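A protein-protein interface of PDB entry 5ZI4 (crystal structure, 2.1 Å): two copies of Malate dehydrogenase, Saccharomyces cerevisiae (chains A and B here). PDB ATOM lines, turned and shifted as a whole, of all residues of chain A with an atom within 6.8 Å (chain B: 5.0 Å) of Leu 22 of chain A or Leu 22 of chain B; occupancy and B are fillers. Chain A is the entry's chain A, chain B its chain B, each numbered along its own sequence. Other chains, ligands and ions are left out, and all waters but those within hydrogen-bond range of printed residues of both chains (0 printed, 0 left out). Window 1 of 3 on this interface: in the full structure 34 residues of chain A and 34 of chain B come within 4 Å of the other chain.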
ATOM      1  N   GLN A  17      32.208 -23.098   3.334  1.00  0.00           N
ATOM      2  CA  GLN A  17      31.340 -24.211   3.815  1.00  0.00           C
ATOM      3  C   GLN A  17      29.952 -24.089   3.244  1.00  0.00           C
ATOM      4  O   GLN A  17      29.492 -25.046   2.579  1.00  0.00           O
ATOM      5  CB  GLN A  17      31.223 -24.286   5.349  1.00  0.00           C
ATOM      6  CG  GLN A  17      32.462 -24.783   5.983  1.00  0.00           C
ATOM      7  CD  GLN A  17      32.281 -25.147   7.452  1.00  0.00           C
ATOM      8  OE1 GLN A  17      31.352 -25.836   7.836  1.00  0.00           O
ATOM      9  NE2 GLN A  17      33.208 -24.690   8.270  1.00  0.00           N
ATOM     10  N   PRO A  18      29.298 -22.914   3.445  1.00  0.00           N
ATOM     11  CA  PRO A  18      28.026 -22.734   2.790  1.00  0.00           C
ATOM     12  C   PRO A  18      28.102 -22.834   1.260  1.00  0.00           C
ATOM     13  O   PRO A  18      27.157 -23.367   0.624  1.00  0.00           O
ATOM     14  CB  PRO A  18      27.540 -21.375   3.264  1.00  0.00           C
ATOM     15  CG  PRO A  18      28.722 -20.661   3.757  1.00  0.00           C
ATOM     16  CD  PRO A  18      29.706 -21.701   4.194  1.00  0.00           C
ATOM     17  N   LEU A  19      29.194 -22.375   0.675  1.00  0.00           N
ATOM     18  CA  LEU A  19      29.334 -22.488  -0.760  1.00  0.00           C
ATOM     19  C   LEU A  19      29.342 -23.951  -1.201  1.00  0.00           C
ATOM     20  O   LEU A  19      28.747 -24.300  -2.214  1.00  0.00           O
ATOM     21  CB  LEU A  19      30.621 -21.826  -1.254  1.00  0.00           C
ATOM     22  CG  LEU A  19      30.894 -21.851  -2.788  1.00  0.00           C
ATOM     23  CD1 LEU A  19      29.845 -21.146  -3.613  1.00  0.00           C
ATOM     24  CD2 LEU A  19      32.231 -21.158  -2.986  1.00  0.00           C
ATOM     25  N   SER A  20      30.102 -24.762  -0.475  1.00  0.00           N
ATOM     26  CA  SER A  20      30.140 -26.196  -0.700  1.00  0.00           C
ATOM     27  C   SER A  20      28.798 -26.901  -0.543  1.00  0.00           C
ATOM     28  O   SER A  20      28.458 -27.749  -1.377  1.00  0.00           O
ATOM     29  CB  SER A  20      31.170 -26.862   0.183  1.00  0.00           C
ATOM     30  OG  SER A  20      32.433 -26.250   0.014  1.00  0.00           O
ATOM     31  N   LEU A  21      28.051 -26.563   0.512  1.00  0.00           N
ATOM     32  CA  LEU A  21      26.676 -27.089   0.698  1.00  0.00           C
ATOM     33  C   LEU A  21      25.792 -26.795  -0.553  1.00  0.00           C
ATOM     34  O   LEU A  21      25.150 -27.682  -1.104  1.00  0.00           O
ATOM     35  CB  LEU A  21      26.085 -26.487   1.985  1.00  0.00           C
ATOM     36  CG  LEU A  21      24.572 -26.603   2.135  1.00  0.00           C
ATOM     37  CD1 LEU A  21      24.121 -28.054   2.133  1.00  0.00           C
ATOM     38  CD2 LEU A  21      24.156 -25.856   3.367  1.00  0.00           C
ATOM     39  N   LEU A  22      25.819 -25.556  -1.043  1.00  0.00           N
ATOM     40  CA  LEU A  22      24.984 -25.195  -2.194  1.00  0.00           C
ATOM     41  C   LEU A  22      25.481 -25.938  -3.401  1.00  0.00           C
ATOM     42  O   LEU A  22      24.664 -26.450  -4.174  1.00  0.00           O
ATOM     43  CB  LEU A  22      24.916 -23.676  -2.417  1.00  0.00           C
ATOM     44  CG  LEU A  22      24.205 -22.949  -1.293  1.00  0.00           C
ATOM     45  CD1 LEU A  22      24.195 -21.471  -1.619  1.00  0.00           C
ATOM     46  CD2 LEU A  22      22.763 -23.413  -1.112  1.00  0.00           C
ATOM     47  N   LEU A  23      26.807 -26.092  -3.533  1.00  0.00           N
ATOM     48  CA  LEU A  23      27.311 -26.822  -4.666  1.00  0.00           C
ATOM     49  C   LEU A  23      26.933 -28.276  -4.547  1.00  0.00           C
ATOM     50  O   LEU A  23      26.715 -28.939  -5.581  1.00  0.00           O
ATOM     51  CB  LEU A  23      28.842 -26.636  -4.891  1.00  0.00           C
ATOM     52  CG  LEU A  23      29.248 -25.573  -5.915  1.00  0.00           C
ATOM     53  CD1 LEU A  23      29.020 -26.126  -7.310  1.00  0.00           C
ATOM     54  CD2 LEU A  23      28.537 -24.267  -5.746  1.00  0.00           C
ATOM     55  N   LYS A  24      26.848 -28.817  -3.330  1.00  0.00           N
ATOM     56  CA  LYS A  24      26.385 -30.225  -3.198  1.00  0.00           C
ATOM     57  C   LYS A  24      24.979 -30.454  -3.784  1.00  0.00           C
ATOM     58  O   LYS A  24      24.628 -31.561  -4.151  1.00  0.00           O
ATOM     59  CB  LYS A  24      26.395 -30.646  -1.731  1.00  0.00           C
ATOM     60  CG  LYS A  24      26.034 -32.122  -1.427  1.00  0.00           C
ATOM     61  CD  LYS A  24      27.000 -33.120  -2.022  1.00  0.00           C
ATOM     62  CE  LYS A  24      26.579 -34.558  -1.754  1.00  0.00           C
ATOM     63  NZ  LYS A  24      25.715 -35.127  -2.782  1.00  0.00           N
ATOM     64  N   LEU A  25      24.150 -29.427  -3.740  1.00  0.00           N
ATOM     65  CA  LEU A  25      22.776 -29.499  -4.220  1.00  0.00           C
ATOM     66  C   LEU A  25      22.620 -29.317  -5.727  1.00  0.00           C
ATOM     67  O   LEU A  25      21.520 -29.449  -6.227  1.00  0.00           O
ATOM     68  CB  LEU A  25      21.927 -28.385  -3.585  1.00  0.00           C
ATOM     69  CG  LEU A  25      21.929 -28.250  -2.075  1.00  0.00           C
ATOM     70  CD1 LEU A  25      20.859 -27.227  -1.641  1.00  0.00           C
ATOM     71  CD2 LEU A  25      21.778 -29.619  -1.420  1.00  0.00           C
ATOM     72  N   SER A  26      23.679 -28.921  -6.430  1.00  0.00           N
ATOM     73  CA  SER A  26      23.620 -28.751  -7.887  1.00  0.00           C
ATOM     74  C   SER A  26      23.418 -30.102  -8.614  1.00  0.00           C
ATOM     75  O   SER A  26      24.267 -30.999  -8.483  1.00  0.00           O
ATOM     76  CB  SER A  26      24.919 -28.077  -8.399  1.00  0.00           C
ATOM     77  OG  SER A  26      24.851 -27.812  -9.806  1.00  0.00           O
ATOM     78  N   LEU A  32      32.315 -33.559  -6.456  1.00  0.00           N
ATOM     79  CA  LEU A  32      32.547 -32.326  -5.738  1.00  0.00           C
ATOM     80  C   LEU A  32      33.701 -32.620  -4.859  1.00  0.00           C
ATOM     81  O   LEU A  32      33.601 -33.539  -4.030  1.00  0.00           O
ATOM     82  CB  LEU A  32      31.350 -31.922  -4.903  1.00  0.00           C
ATOM     83  CG  LEU A  32      31.479 -30.618  -4.089  1.00  0.00           C
ATOM     84  CD1 LEU A  32      31.976 -29.448  -4.932  1.00  0.00           C
ATOM     85  CD2 LEU A  32      30.127 -30.287  -3.458  1.00  0.00           C
ATOM     86  N   LEU A  47      28.835 -33.328   4.086  1.00  0.00           N
ATOM     87  CA  LEU A  47      28.043 -33.129   2.886  1.00  0.00           C
ATOM     88  C   LEU A  47      27.753 -34.426   2.114  1.00  0.00           C
ATOM     89  O   LEU A  47      26.736 -34.497   1.480  1.00  0.00           O
ATOM     90  CB  LEU A  47      28.669 -32.096   1.968  1.00  0.00           C
ATOM     91  CG  LEU A  47      28.729 -30.697   2.533  1.00  0.00           C
ATOM     92  CD1 LEU A  47      29.596 -29.834   1.648  1.00  0.00           C
ATOM     93  CD2 LEU A  47      27.336 -30.119   2.662  1.00  0.00           C
ATOM     94  N   LEU A 237      27.381 -15.952   3.977  1.00  0.00           N
ATOM     95  CA  LEU A 237      26.227 -16.743   3.497  1.00  0.00           C
ATOM     96  C   LEU A 237      25.626 -16.175   2.185  1.00  0.00           C
ATOM     97  O   LEU A 237      25.335 -16.908   1.269  1.00  0.00           O
ATOM     98  CB  LEU A 237      25.140 -16.733   4.588  1.00  0.00           C
ATOM     99  CG  LEU A 237      25.517 -17.322   5.961  1.00  0.00           C
ATOM    100  CD1 LEU A 237      24.367 -17.257   6.949  1.00  0.00           C
ATOM    101  CD2 LEU A 237      26.034 -18.754   5.818  1.00  0.00           C
ATOM    102  N   MET A 239      27.330 -14.352   0.134  1.00  0.00           N
ATOM    103  CA  MET A 239      28.378 -14.687  -0.832  1.00  0.00           C
ATOM    104  C   MET A 239      28.276 -16.103  -1.329  1.00  0.00           C
ATOM    105  O   MET A 239      28.421 -16.335  -2.500  1.00  0.00           O
ATOM    106  CB  MET A 239      29.810 -14.407  -0.325  1.00  0.00           C
ATOM    107  CG  MET A 239      30.872 -14.767  -1.357  1.00  0.00           C
ATOM    108  SD  MET A 239      30.761 -13.630  -2.782  1.00  0.00           S
ATOM    109  CE  MET A 239      30.649 -14.754  -4.162  1.00  0.00           C
ATOM    110  N   ALA A 240      28.044 -17.073  -0.439  1.00  0.00           N
ATOM    111  CA  ALA A 240      27.938 -18.467  -0.866  1.00  0.00           C
ATOM    112  C   ALA A 240      26.744 -18.596  -1.850  1.00  0.00           C
ATOM    113  O   ALA A 240      26.804 -19.303  -2.889  1.00  0.00           O
ATOM    114  CB  ALA A 240      27.749 -19.362   0.379  1.00  0.00           C
ATOM    115  N   PHE A 241      25.646 -17.928  -1.507  1.00  0.00           N
ATOM    116  CA  PHE A 241      24.505 -17.870  -2.393  1.00  0.00           C
ATOM    117  C   PHE A 241      24.873 -17.309  -3.764  1.00  0.00           C
ATOM    118  O   PHE A 241      24.697 -17.994  -4.735  1.00  0.00           O
ATOM    119  CB  PHE A 241      23.390 -17.045  -1.764  1.00  0.00           C
ATOM    120  CG  PHE A 241      22.253 -16.767  -2.703  1.00  0.00           C
ATOM    121  CD1 PHE A 241      21.321 -17.738  -2.993  1.00  0.00           C
ATOM    122  CD2 PHE A 241      22.146 -15.526  -3.322  1.00  0.00           C
ATOM    123  CE1 PHE A 241      20.294 -17.473  -3.866  1.00  0.00           C
ATOM    124  CE2 PHE A 241      21.100 -15.257  -4.194  1.00  0.00           C
ATOM    125  CZ  PHE A 241      20.184 -16.234  -4.470  1.00  0.00           C
ATOM    126  N   ALA A 242      25.436 -16.083  -3.806  1.00  0.00           N
ATOM    127  CA  ALA A 242      25.795 -15.402  -5.095  1.00  0.00           C
ATOM    128  C   ALA A 242      26.856 -16.156  -5.875  1.00  0.00           C
ATOM    129  O   ALA A 242      26.776 -16.312  -7.109  1.00  0.00           O
ATOM    130  CB  ALA A 242      26.207 -13.939  -4.847  1.00  0.00           C
ATOM    131  N   GLY A 243      27.832 -16.690  -5.153  1.00  0.00           N
ATOM    132  CA  GLY A 243      28.819 -17.590  -5.735  1.00  0.00           C
ATOM    133  C   GLY A 243      28.305 -18.885  -6.325  1.00  0.00           C
ATOM    134  O   GLY A 243      28.757 -19.301  -7.391  1.00  0.00           O
ATOM    135  N   ALA A 244      27.437 -19.567  -5.582  1.00  0.00           N
ATOM    136  CA  ALA A 244      26.764 -20.781  -6.080  1.00  0.00           C
ATOM    137  C   ALA A 244      25.858 -20.515  -7.281  1.00  0.00           C
ATOM    138  O   ALA A 244      25.838 -21.320  -8.203  1.00  0.00           O
ATOM    139  CB  ALA A 244      25.922 -21.420  -4.992  1.00  0.00           C
ATOM    140  N   LYS A 245      25.039 -19.463  -7.235  1.00  0.00           N
ATOM    141  CA  LYS A 245      24.258 -19.068  -8.453  1.00  0.00           C
ATOM    142  C   LYS A 245      25.210 -18.893  -9.614  1.00  0.00           C
ATOM    143  O   LYS A 245      24.991 -19.453 -10.681  1.00  0.00           O
ATOM    144  CB  LYS A 245      23.475 -17.759  -8.289  1.00  0.00           C
ATOM    145  CG  LYS A 245      22.129 -17.914  -7.614  1.00  0.00           C
ATOM    146  CD  LYS A 245      21.046 -18.360  -8.585  1.00  0.00           C
ATOM    147  CE  LYS A 245      19.845 -18.963  -7.864  1.00  0.00           C
ATOM    148  NZ  LYS A 245      19.251 -20.058  -8.680  1.00  0.00           N
ATOM    149  N   GLU A 248      26.529 -22.053 -10.967  1.00  0.00           N
ATOM    150  CA  GLU A 248      25.406 -22.729 -11.635  1.00  0.00           C
ATOM    151  C   GLU A 248      25.254 -22.330 -13.114  1.00  0.00           C
ATOM    152  O   GLU A 248      25.015 -23.220 -13.968  1.00  0.00           O
ATOM    153  CB  GLU A 248      24.089 -22.491 -10.896  1.00  0.00           C
ATOM    154  CG  GLU A 248      23.043 -23.585 -11.088  1.00  0.00           C
ATOM    155  CD  GLU A 248      23.201 -24.790 -10.132  1.00  0.00           C
ATOM    156  OE1 GLU A 248      22.148 -25.295  -9.637  1.00  0.00           O
ATOM    157  OE2 GLU A 248      24.347 -25.272  -9.919  1.00  0.00           O
ATOM    158  N   PRO B  18      23.744 -22.168   8.244  1.00  0.00           N
ATOM    159  CA  PRO B  18      23.314 -22.690   6.950  1.00  0.00           C
ATOM    160  C   PRO B  18      21.825 -23.039   6.875  1.00  0.00           C
ATOM    161  O   PRO B  18      21.245 -23.028   5.741  1.00  0.00           O
ATOM    162  CB  PRO B  18      24.184 -23.937   6.761  1.00  0.00           C
ATOM    163  CG  PRO B  18      24.600 -24.313   8.118  1.00  0.00           C
ATOM    164  CD  PRO B  18      24.855 -22.979   8.790  1.00  0.00           C
ATOM    165  N   LEU B  19      21.226 -23.344   8.036  1.00  0.00           N
ATOM    166  CA  LEU B  19      19.781 -23.489   8.140  1.00  0.00           C
ATOM    167  C   LEU B  19      19.100 -22.170   7.844  1.00  0.00           C
ATOM    168  O   LEU B  19      18.139 -22.142   7.104  1.00  0.00           O
ATOM    169  CB  LEU B  19      19.364 -24.032   9.500  1.00  0.00           C
ATOM    170  CG  LEU B  19      17.842 -24.273   9.696  1.00  0.00           C
ATOM    171  CD1 LEU B  19      17.309 -25.427   8.852  1.00  0.00           C
ATOM    172  CD2 LEU B  19      17.584 -24.563  11.160  1.00  0.00           C
ATOM    173  N   SER B  20      19.601 -21.064   8.404  1.00  0.00           N
ATOM    174  CA  SER B  20      19.058 -19.735   8.150  1.00  0.00           C
ATOM    175  C   SER B  20      19.179 -19.355   6.684  1.00  0.00           C
ATOM    176  O   SER B  20      18.241 -18.842   6.119  1.00  0.00           O
ATOM    177  CB  SER B  20      19.750 -18.721   9.029  1.00  0.00           C
ATOM    178  OG  SER B  20      19.491 -19.055  10.374  1.00  0.00           O
ATOM    179  N   LEU B  21      20.309 -19.696   6.068  1.00  0.00           N
ATOM    180  CA  LEU B  21      20.578 -19.466   4.666  1.00  0.00           C
ATOM    181  C   LEU B  21      19.540 -20.212   3.835  1.00  0.00           C
ATOM    182  O   LEU B  21      18.893 -19.635   2.945  1.00  0.00           O
ATOM    183  CB  LEU B  21      22.000 -19.910   4.270  1.00  0.00           C
ATOM    184  CG  LEU B  21      22.348 -20.028   2.758  1.00  0.00           C
ATOM    185  CD1 LEU B  21      22.098 -18.706   2.046  1.00  0.00           C
ATOM    186  CD2 LEU B  21      23.771 -20.540   2.492  1.00  0.00           C
ATOM    187  N   LEU B  22      19.365 -21.471   4.124  1.00  0.00           N
ATOM    188  CA  LEU B  22      18.450 -22.254   3.302  1.00  0.00           C
ATOM    189  C   LEU B  22      17.001 -21.782   3.435  1.00  0.00           C
ATOM    190  O   LEU B  22      16.305 -21.688   2.438  1.00  0.00           O
ATOM    191  CB  LEU B  22      18.582 -23.728   3.572  1.00  0.00           C
ATOM    192  CG  LEU B  22      19.852 -24.453   3.141  1.00  0.00           C
ATOM    193  CD1 LEU B  22      19.706 -25.938   3.434  1.00  0.00           C
ATOM    194  CD2 LEU B  22      20.136 -24.325   1.634  1.00  0.00           C
ATOM    195  N   LEU B  23      16.588 -21.428   4.641  1.00  0.00           N
ATOM    196  CA  LEU B  23      15.268 -20.795   4.858  1.00  0.00           C
ATOM    197  C   LEU B  23      15.050 -19.439   4.193  1.00  0.00           C
ATOM    198  O   LEU B  23      13.898 -19.112   3.903  1.00  0.00           O
ATOM    199  CB  LEU B  23      14.940 -20.655   6.351  1.00  0.00           C
ATOM    200  CG  LEU B  23      14.182 -21.845   6.983  1.00  0.00           C
ATOM    201  CD1 LEU B  23      12.703 -21.899   6.545  1.00  0.00           C
ATOM    202  CD2 LEU B  23      14.856 -23.168   6.699  1.00  0.00           C
ATOM    203  N   LYS B  24      16.108 -18.642   4.002  1.00  0.00           N
ATOM    204  CA  LYS B  24      16.004 -17.368   3.271  1.00  0.00           C
ATOM    205  C   LYS B  24      15.674 -17.639   1.835  1.00  0.00           C
ATOM    206  O   LYS B  24      15.007 -16.826   1.240  1.00  0.00           O
ATOM    207  CB  LYS B  24      17.252 -16.456   3.399  1.00  0.00           C
ATOM    208  CG  LYS B  24      17.174 -15.113   2.634  1.00  0.00           C
ATOM    209  CD  LYS B  24      16.520 -13.987   3.416  1.00  0.00           C
ATOM    210  CE  LYS B  24      16.332 -12.687   2.623  1.00  0.00           C
ATOM    211  NZ  LYS B  24      15.559 -12.962   1.383  1.00  0.00           N
ATOM    212  N   LEU B  25      16.080 -18.799   1.309  1.00  0.00           N
ATOM    213  CA  LEU B  25      15.760 -19.208  -0.053  1.00  0.00           C
ATOM    214  C   LEU B  25      14.366 -19.818  -0.272  1.00  0.00           C
ATOM    215  O   LEU B  25      14.018 -20.172  -1.404  1.00  0.00           O
ATOM    216  CB  LEU B  25      16.762 -20.268  -0.534  1.00  0.00           C
ATOM    217  CG  LEU B  25      18.244 -19.981  -0.396  1.00  0.00           C
ATOM    218  CD1 LEU B  25      18.996 -21.090  -1.088  1.00  0.00           C
ATOM    219  CD2 LEU B  25      18.588 -18.633  -0.947  1.00  0.00           C
ATOM    220  N   SER B  26      13.577 -19.971   0.780  1.00  0.00           N
ATOM    221  CA  SER B  26      12.275 -20.581   0.648  1.00  0.00           C
ATOM    222  C   SER B  26      11.248 -19.590   0.121  1.00  0.00           C
ATOM    223  O   SER B  26      11.083 -18.555   0.731  1.00  0.00           O
ATOM    224  CB  SER B  26      11.807 -21.063   2.040  1.00  0.00           C
ATOM    225  OG  SER B  26      10.520 -21.637   1.965  1.00  0.00           O
ATOM    226  N   ALA B 240      21.525 -28.905   8.441  1.00  0.00           N
ATOM    227  CA  ALA B 240      20.895 -27.709   7.898  1.00  0.00           C
ATOM    228  C   ALA B 240      19.997 -28.079   6.705  1.00  0.00           C
ATOM    229  O   ALA B 240      18.870 -27.650   6.628  1.00  0.00           O
ATOM    230  CB  ALA B 240      21.926 -26.719   7.425  1.00  0.00           C
ATOM    231  N   PHE B 241      20.528 -28.898   5.810  1.00  0.00           N
ATOM    232  CA  PHE B 241      19.796 -29.354   4.644  1.00  0.00           C
ATOM    233  C   PHE B 241      18.552 -30.105   5.010  1.00  0.00           C
ATOM    234  O   PHE B 241      17.477 -29.772   4.543  1.00  0.00           O
ATOM    235  CB  PHE B 241      20.673 -30.258   3.795  1.00  0.00           C
ATOM    236  CG  PHE B 241      19.926 -30.962   2.695  1.00  0.00           C
ATOM    237  CD1 PHE B 241      19.645 -30.307   1.503  1.00  0.00           C
ATOM    238  CD2 PHE B 241      19.544 -32.290   2.848  1.00  0.00           C
ATOM    239  CE1 PHE B 241      18.970 -30.969   0.474  1.00  0.00           C
ATOM    240  CE2 PHE B 241      18.877 -32.945   1.839  1.00  0.00           C
ATOM    241  CZ  PHE B 241      18.599 -32.291   0.654  1.00  0.00           C
ATOM    242  N   ALA B 244      16.015 -27.927   6.863  1.00  0.00           N
ATOM    243  CA  ALA B 244      15.280 -27.048   5.943  1.00  0.00           C
ATOM    244  C   ALA B 244      14.289 -27.864   5.068  1.00  0.00           C
ATOM    245  O   ALA B 244      13.198 -27.384   4.738  1.00  0.00           O
ATOM    246  CB  ALA B 244      16.228 -26.258   5.075  1.00  0.00           C
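Printed residues of chain B within 4 Å of Pro 18 of chain A: Leu 21.
Of the printed residues of chain B, Leu 21 of chain A touches Pro 18 (3.9 Å).
Leu 22 of chain A touches one residue of chain B.
Of the printed residues of chain B, Leu 237 of chain A touches Leu 21.
Of the printed residues of chain A, Pro 18 of chain B touches Leu 21 (3.9 Å).
Leu 22 of chain B touches just one residue of chain A: Leu 22 (3.9 Å).
The nearest residue of chain B that does not touch Leu 22 of chain A is Leu 21 of chain B (4.2 Å).
The nearest printed residue of chain A that does not touch Leu 22 of chain B is Leu 25 of chain A (4.4 Å).
The nearest printed residue of chain B that does not touch Phe 241 of chain A is Leu 21 of chain B (4.4 Å).
Among the printed residues, pairs that only touch across the chains: Pro 18 of chain A with Leu 21 of chain B (3.9 Å), Leu 21 of chain A with Pro 18 of chain B (3.9 Å), Leu 22 of chain A with Leu 22 of chain B (3.9 Å), Leu 25 of chain A with Phe 241 of chain B (3.6 Å), Leu 237 of chain A with Leu 21 of chain B (3.8 Å) and Phe 241 of chain A with Leu 25 of chain B (3.5 Å).
Hydrophobic or aromatic side chains of chain B within 4 Å of the printed part of chain A: Pro 18, Leu 21, Leu 22, Leu 25 and Phe 241.
Along chain B the printed residues that touch a printed residue of chain A span positions 18 to 241.
Of the 21 printed residues of chain A, 6 touch a printed residue of chain B.
Printed residues of chain A that touch a printed residue of chain B: Pro 18, Leu 21, Leu 22, Leu 25, Leu 237 and Phe 241.
Hydrophobic or aromatic side chains of chain A that line the printed part of chain B: Pro 18, Leu 21, Leu 22, Leu 25 and Phe 241.
Among the printed residues, 6 pairs touch across the chains.
Among the printed residues, no Asp or Glu carboxylate lies within 4 Å of a Lys or Arg side-chain nitrogen of the other chain.
Pro 18 of chain A touches Leu 21 of chain B, and with the chains exchanged Leu 21 of chain A touches Pro 18 of chain B.
Leu 22 of chain A touches its own counterpart, Leu 22 of chain B.
Leu 25 of chain A touches Phe 241 of chain B, and with the chains exchanged Phe 241 of chain A touches Leu 25 of chain B.
Positions printed for both chains: 18, 19, 20, 21, 22, 23, 24, 25, 26, 240, 241 and 244.
Of the 6 pairs that touch across the chains among the printed residues, 5 have their exchanged pair printed and touching as well.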
